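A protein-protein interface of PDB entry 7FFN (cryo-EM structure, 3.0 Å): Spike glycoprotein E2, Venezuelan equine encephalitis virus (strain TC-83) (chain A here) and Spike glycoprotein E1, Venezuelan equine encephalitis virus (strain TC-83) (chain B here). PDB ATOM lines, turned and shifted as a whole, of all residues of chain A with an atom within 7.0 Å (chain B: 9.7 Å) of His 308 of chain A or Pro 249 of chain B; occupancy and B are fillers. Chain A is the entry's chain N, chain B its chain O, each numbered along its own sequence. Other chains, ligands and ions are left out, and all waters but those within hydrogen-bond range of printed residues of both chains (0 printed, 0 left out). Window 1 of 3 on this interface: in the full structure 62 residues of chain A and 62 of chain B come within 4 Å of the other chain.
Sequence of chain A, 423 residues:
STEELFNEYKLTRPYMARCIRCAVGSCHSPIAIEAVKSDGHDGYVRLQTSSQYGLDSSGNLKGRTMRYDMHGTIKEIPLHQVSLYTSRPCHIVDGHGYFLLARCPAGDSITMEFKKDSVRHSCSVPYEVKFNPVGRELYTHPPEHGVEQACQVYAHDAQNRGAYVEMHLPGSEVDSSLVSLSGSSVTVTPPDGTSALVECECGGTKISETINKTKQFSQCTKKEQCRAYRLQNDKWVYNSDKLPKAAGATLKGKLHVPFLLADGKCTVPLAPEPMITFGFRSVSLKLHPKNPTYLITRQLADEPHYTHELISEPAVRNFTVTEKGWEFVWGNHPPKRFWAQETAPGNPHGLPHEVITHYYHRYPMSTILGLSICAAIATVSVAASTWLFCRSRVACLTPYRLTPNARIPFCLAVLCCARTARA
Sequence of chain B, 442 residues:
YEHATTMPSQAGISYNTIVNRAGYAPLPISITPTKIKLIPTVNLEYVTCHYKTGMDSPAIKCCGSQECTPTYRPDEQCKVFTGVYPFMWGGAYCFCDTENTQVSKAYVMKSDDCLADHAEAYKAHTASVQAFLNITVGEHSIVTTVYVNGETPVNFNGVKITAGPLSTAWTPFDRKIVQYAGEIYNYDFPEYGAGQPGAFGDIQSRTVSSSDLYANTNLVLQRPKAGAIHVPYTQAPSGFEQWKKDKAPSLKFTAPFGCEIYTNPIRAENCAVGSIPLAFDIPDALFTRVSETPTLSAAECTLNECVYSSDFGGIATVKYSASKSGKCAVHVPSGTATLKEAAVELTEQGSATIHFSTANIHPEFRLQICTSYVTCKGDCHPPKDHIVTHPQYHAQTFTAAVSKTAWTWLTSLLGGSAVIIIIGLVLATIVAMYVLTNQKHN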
ATOM      1  N   ARG A 136       9.637  29.634   2.970  1.00  0.00           N
ATOM      2  CA  ARG A 136       9.562  28.221   2.645  1.00  0.00           C
ATOM      3  C   ARG A 136      10.927  27.549   2.586  1.00  0.00           C
ATOM      4  O   ARG A 136      11.051  26.488   1.975  1.00  0.00           O
ATOM      5  CB  ARG A 136       8.827  28.007   1.321  1.00  0.00           C
ATOM      6  CG  ARG A 136       7.313  27.972   1.411  1.00  0.00           C
ATOM      7  CD  ARG A 136       6.687  29.319   1.158  1.00  0.00           C
ATOM      8  NE  ARG A 136       6.967  29.759  -0.201  1.00  0.00           N
ATOM      9  CZ  ARG A 136       6.707  30.975  -0.662  1.00  0.00           C
ATOM     10  NH1 ARG A 136       6.143  31.871   0.126  1.00  0.00           N
ATOM     11  NH2 ARG A 136       7.008  31.291  -1.908  1.00  0.00           N
ATOM     12  N   TYR A 294      11.426  23.749   0.674  1.00  0.00           N
ATOM     13  CA  TYR A 294      10.141  23.216   0.248  1.00  0.00           C
ATOM     14  C   TYR A 294       9.885  23.446  -1.235  1.00  0.00           C
ATOM     15  O   TYR A 294      10.193  24.505  -1.781  1.00  0.00           O
ATOM     16  CB  TYR A 294       8.998  23.850   1.032  1.00  0.00           C
ATOM     17  CG  TYR A 294       8.848  23.380   2.450  1.00  0.00           C
ATOM     18  CD1 TYR A 294       8.287  22.149   2.731  1.00  0.00           C
ATOM     19  CD2 TYR A 294       9.218  24.191   3.508  1.00  0.00           C
ATOM     20  CE1 TYR A 294       8.131  21.720   4.022  1.00  0.00           C
ATOM     21  CE2 TYR A 294       9.062  23.772   4.806  1.00  0.00           C
ATOM     22  CZ  TYR A 294       8.521  22.534   5.055  1.00  0.00           C
ATOM     23  OH  TYR A 294       8.366  22.115   6.355  1.00  0.00           O
ATOM     24  N   LEU A 295       9.269  22.452  -1.866  1.00  0.00           N
ATOM     25  CA  LEU A 295       8.825  22.497  -3.256  1.00  0.00           C
ATOM     26  C   LEU A 295       7.320  22.291  -3.285  1.00  0.00           C
ATOM     27  O   LEU A 295       6.837  21.220  -2.914  1.00  0.00           O
ATOM     28  CB  LEU A 295       9.497  21.401  -4.075  1.00  0.00           C
ATOM     29  CG  LEU A 295       9.041  21.291  -5.525  1.00  0.00           C
ATOM     30  CD1 LEU A 295       9.568  22.413  -6.363  1.00  0.00           C
ATOM     31  CD2 LEU A 295       9.411  19.959  -6.115  1.00  0.00           C
ATOM     32  N   ILE A 296       6.581  23.292  -3.744  1.00  0.00           N
ATOM     33  CA  ILE A 296       5.129  23.235  -3.741  1.00  0.00           C
ATOM     34  C   ILE A 296       4.663  23.344  -5.181  1.00  0.00           C
ATOM     35  O   ILE A 296       4.904  24.360  -5.836  1.00  0.00           O
ATOM     36  CB  ILE A 296       4.502  24.338  -2.885  1.00  0.00           C
ATOM     37  CG1 ILE A 296       4.961  24.231  -1.436  1.00  0.00           C
ATOM     38  CG2 ILE A 296       3.017  24.225  -2.960  1.00  0.00           C
ATOM     39  CD1 ILE A 296       4.578  25.407  -0.604  1.00  0.00           C
ATOM     40  N   THR A 297       4.006  22.298  -5.681  1.00  0.00           N
ATOM     41  CA  THR A 297       3.501  22.265  -7.046  1.00  0.00           C
ATOM     42  C   THR A 297       2.013  21.964  -7.034  1.00  0.00           C
ATOM     43  O   THR A 297       1.528  21.258  -6.152  1.00  0.00           O
ATOM     44  CB  THR A 297       4.200  21.201  -7.894  1.00  0.00           C
ATOM     45  OG1 THR A 297       3.866  19.908  -7.397  1.00  0.00           O
ATOM     46  CG2 THR A 297       5.699  21.348  -7.850  1.00  0.00           C
ATOM     47  N   TYR A 306      -2.222  18.671  -5.694  1.00  0.00           N
ATOM     48  CA  TYR A 306      -1.057  19.430  -5.271  1.00  0.00           C
ATOM     49  C   TYR A 306      -0.043  18.526  -4.586  1.00  0.00           C
ATOM     50  O   TYR A 306      -0.360  17.439  -4.104  1.00  0.00           O
ATOM     51  CB  TYR A 306      -1.443  20.579  -4.338  1.00  0.00           C
ATOM     52  CG  TYR A 306      -1.823  20.175  -2.936  1.00  0.00           C
ATOM     53  CD1 TYR A 306      -3.103  19.735  -2.652  1.00  0.00           C
ATOM     54  CD2 TYR A 306      -0.922  20.294  -1.883  1.00  0.00           C
ATOM     55  CE1 TYR A 306      -3.462  19.378  -1.372  1.00  0.00           C
ATOM     56  CE2 TYR A 306      -1.270  19.936  -0.601  1.00  0.00           C
ATOM     57  CZ  TYR A 306      -2.543  19.482  -0.353  1.00  0.00           C
ATOM     58  OH  TYR A 306      -2.911  19.127   0.922  1.00  0.00           O
ATOM     59  N   THR A 307       1.198  18.993  -4.559  1.00  0.00           N
ATOM     60  CA  THR A 307       2.304  18.233  -4.007  1.00  0.00           C
ATOM     61  C   THR A 307       3.135  19.186  -3.165  1.00  0.00           C
ATOM     62  O   THR A 307       3.264  20.363  -3.500  1.00  0.00           O
ATOM     63  CB  THR A 307       3.130  17.594  -5.129  1.00  0.00           C
ATOM     64  OG1 THR A 307       2.261  16.844  -5.979  1.00  0.00           O
ATOM     65  CG2 THR A 307       4.159  16.642  -4.587  1.00  0.00           C
ATOM     66  N   HIS A 308       3.663  18.686  -2.054  1.00  0.00           N
ATOM     67  CA  HIS A 308       4.368  19.490  -1.068  1.00  0.00           C
ATOM     68  C   HIS A 308       5.468  18.633  -0.475  1.00  0.00           C
ATOM     69  O   HIS A 308       5.189  17.549   0.041  1.00  0.00           O
ATOM     70  CB  HIS A 308       3.398  19.952   0.010  1.00  0.00           C
ATOM     71  CG  HIS A 308       4.035  20.687   1.138  1.00  0.00           C
ATOM     72  ND1 HIS A 308       4.420  22.005   1.046  1.00  0.00           N
ATOM     73  CD2 HIS A 308       4.328  20.296   2.397  1.00  0.00           C
ATOM     74  CE1 HIS A 308       4.927  22.391   2.200  1.00  0.00           C
ATOM     75  NE2 HIS A 308       4.885  21.373   3.038  1.00  0.00           N
ATOM     76  N   GLU A 309       6.711  19.099  -0.559  1.00  0.00           N
ATOM     77  CA  GLU A 309       7.838  18.234  -0.249  1.00  0.00           C
ATOM     78  C   GLU A 309       9.040  19.053   0.190  1.00  0.00           C
ATOM     79  O   GLU A 309       9.468  19.954  -0.530  1.00  0.00           O
ATOM     80  CB  GLU A 309       8.187  17.385  -1.465  1.00  0.00           C
ATOM     81  CG  GLU A 309       9.301  16.409  -1.240  1.00  0.00           C
ATOM     82  CD  GLU A 309       9.540  15.543  -2.449  1.00  0.00           C
ATOM     83  OE1 GLU A 309       8.831  15.739  -3.455  1.00  0.00           O
ATOM     84  OE2 GLU A 309      10.434  14.675  -2.395  1.00  0.00           O
ATOM     85  N   LEU A 310       9.566  18.740   1.369  1.00  0.00           N
ATOM     86  CA  LEU A 310      10.767  19.385   1.888  1.00  0.00           C
ATOM     87  C   LEU A 310      11.985  18.682   1.306  1.00  0.00           C
ATOM     88  O   LEU A 310      12.315  17.563   1.705  1.00  0.00           O
ATOM     89  CB  LEU A 310      10.802  19.344   3.412  1.00  0.00           C
ATOM     90  CG  LEU A 310      12.056  19.953   4.031  1.00  0.00           C
ATOM     91  CD1 LEU A 310      12.166  21.416   3.688  1.00  0.00           C
ATOM     92  CD2 LEU A 310      12.082  19.761   5.526  1.00  0.00           C
ATOM     93  N   VAL B 178      -9.930  29.865   8.471  1.00  0.00           N
ATOM     94  CA  VAL B 178      -8.995  30.363   9.466  1.00  0.00           C
ATOM     95  C   VAL B 178      -7.977  31.242   8.763  1.00  0.00           C
ATOM     96  O   VAL B 178      -7.270  30.775   7.867  1.00  0.00           O
ATOM     97  CB  VAL B 178      -8.287  29.221  10.206  1.00  0.00           C
ATOM     98  CG1 VAL B 178      -7.236  29.772  11.123  1.00  0.00           C
ATOM     99  CG2 VAL B 178      -9.281  28.399  10.975  1.00  0.00           C
ATOM    100  N   GLU B 183      -2.011  34.314   5.632  1.00  0.00           N
ATOM    101  CA  GLU B 183      -2.503  33.234   4.798  1.00  0.00           C
ATOM    102  C   GLU B 183      -3.831  32.738   5.345  1.00  0.00           C
ATOM    103  O   GLU B 183      -4.201  33.005   6.483  1.00  0.00           O
ATOM    104  CB  GLU B 183      -1.474  32.107   4.720  1.00  0.00           C
ATOM    105  CG  GLU B 183      -0.220  32.525   3.983  1.00  0.00           C
ATOM    106  CD  GLU B 183       0.824  31.440   3.933  1.00  0.00           C
ATOM    107  OE1 GLU B 183       0.606  30.382   4.555  1.00  0.00           O
ATOM    108  OE2 GLU B 183       1.872  31.644   3.282  1.00  0.00           O
ATOM    109  N   ILE B 184      -4.555  32.016   4.499  1.00  0.00           N
ATOM    110  CA  ILE B 184      -5.932  31.633   4.763  1.00  0.00           C
ATOM    111  C   ILE B 184      -6.029  30.123   4.655  1.00  0.00           C
ATOM    112  O   ILE B 184      -5.630  29.547   3.643  1.00  0.00           O
ATOM    113  CB  ILE B 184      -6.898  32.331   3.791  1.00  0.00           C
ATOM    114  CG1 ILE B 184      -6.928  33.822   4.107  1.00  0.00           C
ATOM    115  CG2 ILE B 184      -8.272  31.723   3.845  1.00  0.00           C
ATOM    116  CD1 ILE B 184      -7.553  34.644   3.059  1.00  0.00           C
ATOM    117  N   TYR B 185      -6.526  29.482   5.704  1.00  0.00           N
ATOM    118  CA  TYR B 185      -6.550  28.031   5.796  1.00  0.00           C
ATOM    119  C   TYR B 185      -7.987  27.556   5.837  1.00  0.00           C
ATOM    120  O   TYR B 185      -8.846  28.194   6.446  1.00  0.00           O
ATOM    121  CB  TYR B 185      -5.812  27.548   7.035  1.00  0.00           C
ATOM    122  CG  TYR B 185      -4.341  27.837   7.001  1.00  0.00           C
ATOM    123  CD1 TYR B 185      -3.462  26.964   6.401  1.00  0.00           C
ATOM    124  CD2 TYR B 185      -3.839  29.001   7.542  1.00  0.00           C
ATOM    125  CE1 TYR B 185      -2.125  27.227   6.372  1.00  0.00           C
ATOM    126  CE2 TYR B 185      -2.507  29.271   7.517  1.00  0.00           C
ATOM    127  CZ  TYR B 185      -1.653  28.387   6.927  1.00  0.00           C
ATOM    128  OH  TYR B 185      -0.313  28.677   6.896  1.00  0.00           O
ATOM    129  N   ASN B 186      -8.247  26.436   5.183  1.00  0.00           N
ATOM    130  CA  ASN B 186      -9.609  25.964   4.997  1.00  0.00           C
ATOM    131  C   ASN B 186      -9.899  24.887   6.042  1.00  0.00           C
ATOM    132  O   ASN B 186     -10.096  23.714   5.741  1.00  0.00           O
ATOM    133  CB  ASN B 186      -9.778  25.444   3.573  1.00  0.00           C
ATOM    134  CG  ASN B 186     -11.169  25.637   3.049  1.00  0.00           C
ATOM    135  OD1 ASN B 186     -12.010  26.212   3.721  1.00  0.00           O
ATOM    136  ND2 ASN B 186     -11.413  25.184   1.833  1.00  0.00           N
ATOM    137  N   TYR B 187      -9.916  25.322   7.298  1.00  0.00           N
ATOM    138  CA  TYR B 187      -9.965  24.442   8.456  1.00  0.00           C
ATOM    139  C   TYR B 187     -11.386  24.361   8.998  1.00  0.00           C
ATOM    140  O   TYR B 187     -12.218  25.236   8.749  1.00  0.00           O
ATOM    141  CB  TYR B 187      -9.008  24.946   9.542  1.00  0.00           C
ATOM    142  CG  TYR B 187      -8.798  24.001  10.701  1.00  0.00           C
ATOM    143  CD1 TYR B 187      -8.002  22.879  10.563  1.00  0.00           C
ATOM    144  CD2 TYR B 187      -9.403  24.230  11.925  1.00  0.00           C
ATOM    145  CE1 TYR B 187      -7.817  22.011  11.607  1.00  0.00           C
ATOM    146  CE2 TYR B 187      -9.222  23.365  12.974  1.00  0.00           C
ATOM    147  CZ  TYR B 187      -8.427  22.259  12.809  1.00  0.00           C
ATOM    148  OH  TYR B 187      -8.238  21.398  13.861  1.00  0.00           O
ATOM    149  N   TRP B 243      -1.335  23.306  16.059  1.00  0.00           N
ATOM    150  CA  TRP B 243      -1.908  23.594  14.748  1.00  0.00           C
ATOM    151  C   TRP B 243      -0.863  24.160  13.807  1.00  0.00           C
ATOM    152  O   TRP B 243      -0.846  23.820  12.621  1.00  0.00           O
ATOM    153  CB  TRP B 243      -3.053  24.587  14.872  1.00  0.00           C
ATOM    154  CG  TRP B 243      -3.688  24.909  13.563  1.00  0.00           C
ATOM    155  CD1 TRP B 243      -4.445  24.083  12.801  1.00  0.00           C
ATOM    156  CD2 TRP B 243      -3.597  26.141  12.847  1.00  0.00           C
ATOM    157  NE1 TRP B 243      -4.852  24.724  11.666  1.00  0.00           N
ATOM    158  CE2 TRP B 243      -4.337  25.991  11.668  1.00  0.00           C
ATOM    159  CE3 TRP B 243      -2.965  27.360  13.090  1.00  0.00           C
ATOM    160  CZ2 TRP B 243      -4.462  27.006  10.738  1.00  0.00           C
ATOM    161  CZ3 TRP B 243      -3.088  28.361  12.164  1.00  0.00           C
ATOM    162  CH2 TRP B 243      -3.835  28.182  11.006  1.00  0.00           C
ATOM    163  N   LYS B 244       0.002  25.038  14.318  1.00  0.00           N
ATOM    164  CA  LYS B 244       1.067  25.605  13.500  1.00  0.00           C
ATOM    165  C   LYS B 244       2.063  24.549  13.055  1.00  0.00           C
ATOM    166  O   LYS B 244       2.603  24.634  11.947  1.00  0.00           O
ATOM    167  CB  LYS B 244       1.775  26.712  14.269  1.00  0.00           C
ATOM    168  CG  LYS B 244       1.001  27.995  14.360  1.00  0.00           C
ATOM    169  CD  LYS B 244       1.617  28.914  15.386  1.00  0.00           C
ATOM    170  CE  LYS B 244       3.020  29.340  15.033  1.00  0.00           C
ATOM    171  NZ  LYS B 244       3.068  30.221  13.849  1.00  0.00           N
ATOM    172  N   LYS B 245       2.335  23.551  13.895  1.00  0.00           N
ATOM    173  CA  LYS B 245       3.254  22.501  13.467  1.00  0.00           C
ATOM    174  C   LYS B 245       2.627  21.594  12.419  1.00  0.00           C
ATOM    175  O   LYS B 245       3.318  21.112  11.516  1.00  0.00           O
ATOM    176  CB  LYS B 245       3.705  21.657  14.648  1.00  0.00           C
ATOM    177  CG  LYS B 245       4.634  22.316  15.623  1.00  0.00           C
ATOM    178  CD  LYS B 245       5.052  21.273  16.636  1.00  0.00           C
ATOM    179  CE  LYS B 245       5.933  21.843  17.714  1.00  0.00           C
ATOM    180  NZ  LYS B 245       6.323  20.785  18.677  1.00  0.00           N
ATOM    181  N   ASP B 246       1.328  21.335  12.530  1.00  0.00           N
ATOM    182  CA  ASP B 246       0.643  20.370  11.673  1.00  0.00           C
ATOM    183  C   ASP B 246      -0.231  21.047  10.631  1.00  0.00           C
ATOM    184  O   ASP B 246      -1.306  20.543  10.297  1.00  0.00           O
ATOM    185  CB  ASP B 246      -0.186  19.419  12.521  1.00  0.00           C
ATOM    186  CG  ASP B 246       0.667  18.541  13.404  1.00  0.00           C
ATOM    187  OD1 ASP B 246       1.833  18.293  13.036  1.00  0.00           O
ATOM    188  OD2 ASP B 246       0.177  18.094  14.461  1.00  0.00           O
ATOM    189  N   LYS B 247       0.193  22.193  10.114  1.00  0.00           N
ATOM    190  CA  LYS B 247      -0.524  22.827   9.021  1.00  0.00           C
ATOM    191  C   LYS B 247      -0.372  22.024   7.741  1.00  0.00           C
ATOM    192  O   LYS B 247       0.717  21.551   7.409  1.00  0.00           O
ATOM    193  CB  LYS B 247       0.008  24.227   8.755  1.00  0.00           C
ATOM    194  CG  LYS B 247      -0.294  25.279   9.756  1.00  0.00           C
ATOM    195  CD  LYS B 247       0.411  26.531   9.316  1.00  0.00           C
ATOM    196  CE  LYS B 247       0.254  27.621  10.316  1.00  0.00           C
ATOM    197  NZ  LYS B 247       1.066  28.776   9.895  1.00  0.00           N
ATOM    198  N   ALA B 248      -1.468  21.899   7.011  1.00  0.00           N
ATOM    199  CA  ALA B 248      -1.382  21.710   5.586  1.00  0.00           C
ATOM    200  C   ALA B 248      -0.952  23.033   4.958  1.00  0.00           C
ATOM    201  O   ALA B 248      -1.057  24.081   5.597  1.00  0.00           O
ATOM    202  CB  ALA B 248      -2.733  21.250   5.047  1.00  0.00           C
ATOM    203  N   PRO B 249      -0.430  23.020   3.728  1.00  0.00           N
ATOM    204  CA  PRO B 249      -0.159  24.291   3.048  1.00  0.00           C
ATOM    205  C   PRO B 249      -1.422  25.107   2.837  1.00  0.00           C
ATOM    206  O   PRO B 249      -2.536  24.586   2.801  1.00  0.00           O
ATOM    207  CB  PRO B 249       0.450  23.856   1.714  1.00  0.00           C
ATOM    208  CG  PRO B 249       1.059  22.563   2.004  1.00  0.00           C
ATOM    209  CD  PRO B 249       0.168  21.891   2.997  1.00  0.00           C
ATOM    210  N   SER B 250      -1.230  26.415   2.691  1.00  0.00           N
ATOM    211  CA  SER B 250      -2.335  27.355   2.738  1.00  0.00           C
ATOM    212  C   SER B 250      -3.174  27.265   1.473  1.00  0.00           C
ATOM    213  O   SER B 250      -2.915  26.475   0.568  1.00  0.00           O
ATOM    214  CB  SER B 250      -1.816  28.770   2.943  1.00  0.00           C
ATOM    215  OG  SER B 250      -2.889  29.688   2.931  1.00  0.00           O
ATOM    216  N   LEU B 251      -4.200  28.098   1.406  1.00  0.00           N
ATOM    217  CA  LEU B 251      -5.123  28.002   0.290  1.00  0.00           C
ATOM    218  C   LEU B 251      -4.581  28.670  -0.963  1.00  0.00           C
ATOM    219  O   LEU B 251      -5.100  28.416  -2.050  1.00  0.00           O
ATOM    220  CB  LEU B 251      -6.467  28.598   0.699  1.00  0.00           C
ATOM    221  CG  LEU B 251      -7.751  28.304  -0.048  1.00  0.00           C
ATOM    222  CD1 LEU B 251      -7.974  26.825  -0.003  1.00  0.00           C
ATOM    223  CD2 LEU B 251      -8.862  29.004   0.674  1.00  0.00           C
ATOM    224  N   LYS B 252      -3.523  29.471  -0.850  1.00  0.00           N
ATOM    225  CA  LYS B 252      -2.811  29.977  -2.016  1.00  0.00           C
ATOM    226  C   LYS B 252      -1.888  28.943  -2.641  1.00  0.00           C
ATOM    227  O   LYS B 252      -1.210  29.263  -3.618  1.00  0.00           O
ATOM    228  CB  LYS B 252      -2.000  31.215  -1.646  1.00  0.00           C
ATOM    229  CG  LYS B 252      -0.898  30.938  -0.657  1.00  0.00           C
ATOM    230  CD  LYS B 252      -0.192  32.203  -0.236  1.00  0.00           C
ATOM    231  CE  LYS B 252       0.664  32.748  -1.339  1.00  0.00           C
ATOM    232  NZ  LYS B 252       1.443  33.919  -0.875  1.00  0.00           N
ATOM    233  N   PHE B 253      -1.833  27.725  -2.103  1.00  0.00           N
ATOM    234  CA  PHE B 253      -1.052  26.653  -2.693  1.00  0.00           C
ATOM    235  C   PHE B 253      -1.876  25.439  -3.081  1.00  0.00           C
ATOM    236  O   PHE B 253      -1.393  24.617  -3.863  1.00  0.00           O
ATOM    237  CB  PHE B 253       0.053  26.194  -1.731  1.00  0.00           C
ATOM    238  CG  PHE B 253       1.055  27.257  -1.409  1.00  0.00           C
ATOM    239  CD1 PHE B 253       2.031  27.606  -2.318  1.00  0.00           C
ATOM    240  CD2 PHE B 253       1.029  27.902  -0.193  1.00  0.00           C
ATOM    241  CE1 PHE B 253       2.952  28.581  -2.023  1.00  0.00           C
ATOM    242  CE2 PHE B 253       1.955  28.871   0.105  1.00  0.00           C
ATOM    243  CZ  PHE B 253       2.907  29.216  -0.814  1.00  0.00           C
ATOM    244  N   THR B 254      -3.096  25.292  -2.565  1.00  0.00           N
ATOM    245  CA  THR B 254      -3.896  24.097  -2.796  1.00  0.00           C
ATOM    246  C   THR B 254      -5.225  24.389  -3.475  1.00  0.00           C
ATOM    247  O   THR B 254      -6.056  23.484  -3.584  1.00  0.00           O
ATOM    248  CB  THR B 254      -4.177  23.363  -1.481  1.00  0.00           C
ATOM    249  OG1 THR B 254      -5.052  24.155  -0.677  1.00  0.00           O
ATOM    250  CG2 THR B 254      -2.910  23.135  -0.703  1.00  0.00           C
ATOM    251  N   ALA B 255      -5.456  25.617  -3.938  1.00  0.00           N
ATOM    252  CA  ALA B 255      -6.801  25.829  -4.459  1.00  0.00           C
ATOM    253  C   ALA B 255      -6.841  25.597  -5.963  1.00  0.00           C
ATOM    254  O   ALA B 255      -5.915  25.985  -6.671  1.00  0.00           O
ATOM    255  CB  ALA B 255      -7.283  27.240  -4.160  1.00  0.00           C
ATOM    256  N   ILE B 261      -5.132  33.386  -3.509  1.00  0.00           N
ATOM    257  CA  ILE B 261      -5.830  33.720  -2.272  1.00  0.00           C
ATOM    258  C   ILE B 261      -5.100  34.874  -1.597  1.00  0.00           C
ATOM    259  O   ILE B 261      -3.975  34.711  -1.125  1.00  0.00           O
ATOM    260  CB  ILE B 261      -5.919  32.508  -1.339  1.00  0.00           C
ATOM    261  CG1 ILE B 261      -6.645  31.359  -2.027  1.00  0.00           C
ATOM    262  CG2 ILE B 261      -6.626  32.888  -0.079  1.00  0.00           C
ATOM    263  CD1 ILE B 261      -8.071  31.651  -2.339  1.00  0.00           C
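The side-chain hydroxyl (OG1) of Thr 254 of chain B lies within hydrogen-bond range of the backbone carbonyl oxygen (O) of Ser 250 of chain B, at 3.4 Å.
Among the printed residues, merely in contact across the chains: His 308 of chain A with Pro 249 of chain B, Ile 296 of chain A with Phe 253 of chain B and Tyr 306 of chain A with Thr 254 of chain B.
Pro 249 of chain B touches just one residue of chain A: His 308 (3.5 Å).
No residue of chain B comes within 4 Å of Thr 307 of chain A.
Of the printed residues of chain B, Ile 296 of chain A touches Phe 253.
Of the printed residues of chain A, Phe 253 of chain B touches Ile 296.
Of the printed residues of chain B, Tyr 306 of chain A touches Thr 254.
Printed residues of chain A within 4 Å of Thr 254 of chain B: Tyr 306 (3.6 Å).
Arg 136 of chain A touches none of the printed residues of chain B.
Asp 246 of chain B touches none of the printed residues of chain A.
The nearest residue of chain B that does not touch His 308 of chain A is Lys 247 of chain B (6.0 Å).
Printed residues of chain B that touch a printed residue of chain A: Pro 249, Phe 253 and Thr 254.
Hydrophobic or aromatic side chains of chain B within 4 Å of the printed part of chain A: Pro 249 and Phe 253.
Printed residues of chain A that touch a printed residue of chain B: Ile 296, Tyr 306 and His 308.
Hydrophobic or aromatic side chains of chain A that line the printed part of chain B: Ile 296, Tyr 306 and His 308.
Among the printed residues, no Asp or Glu carboxylate lies within 4 Å of a Lys or Arg side-chain nitrogen of the other chain.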
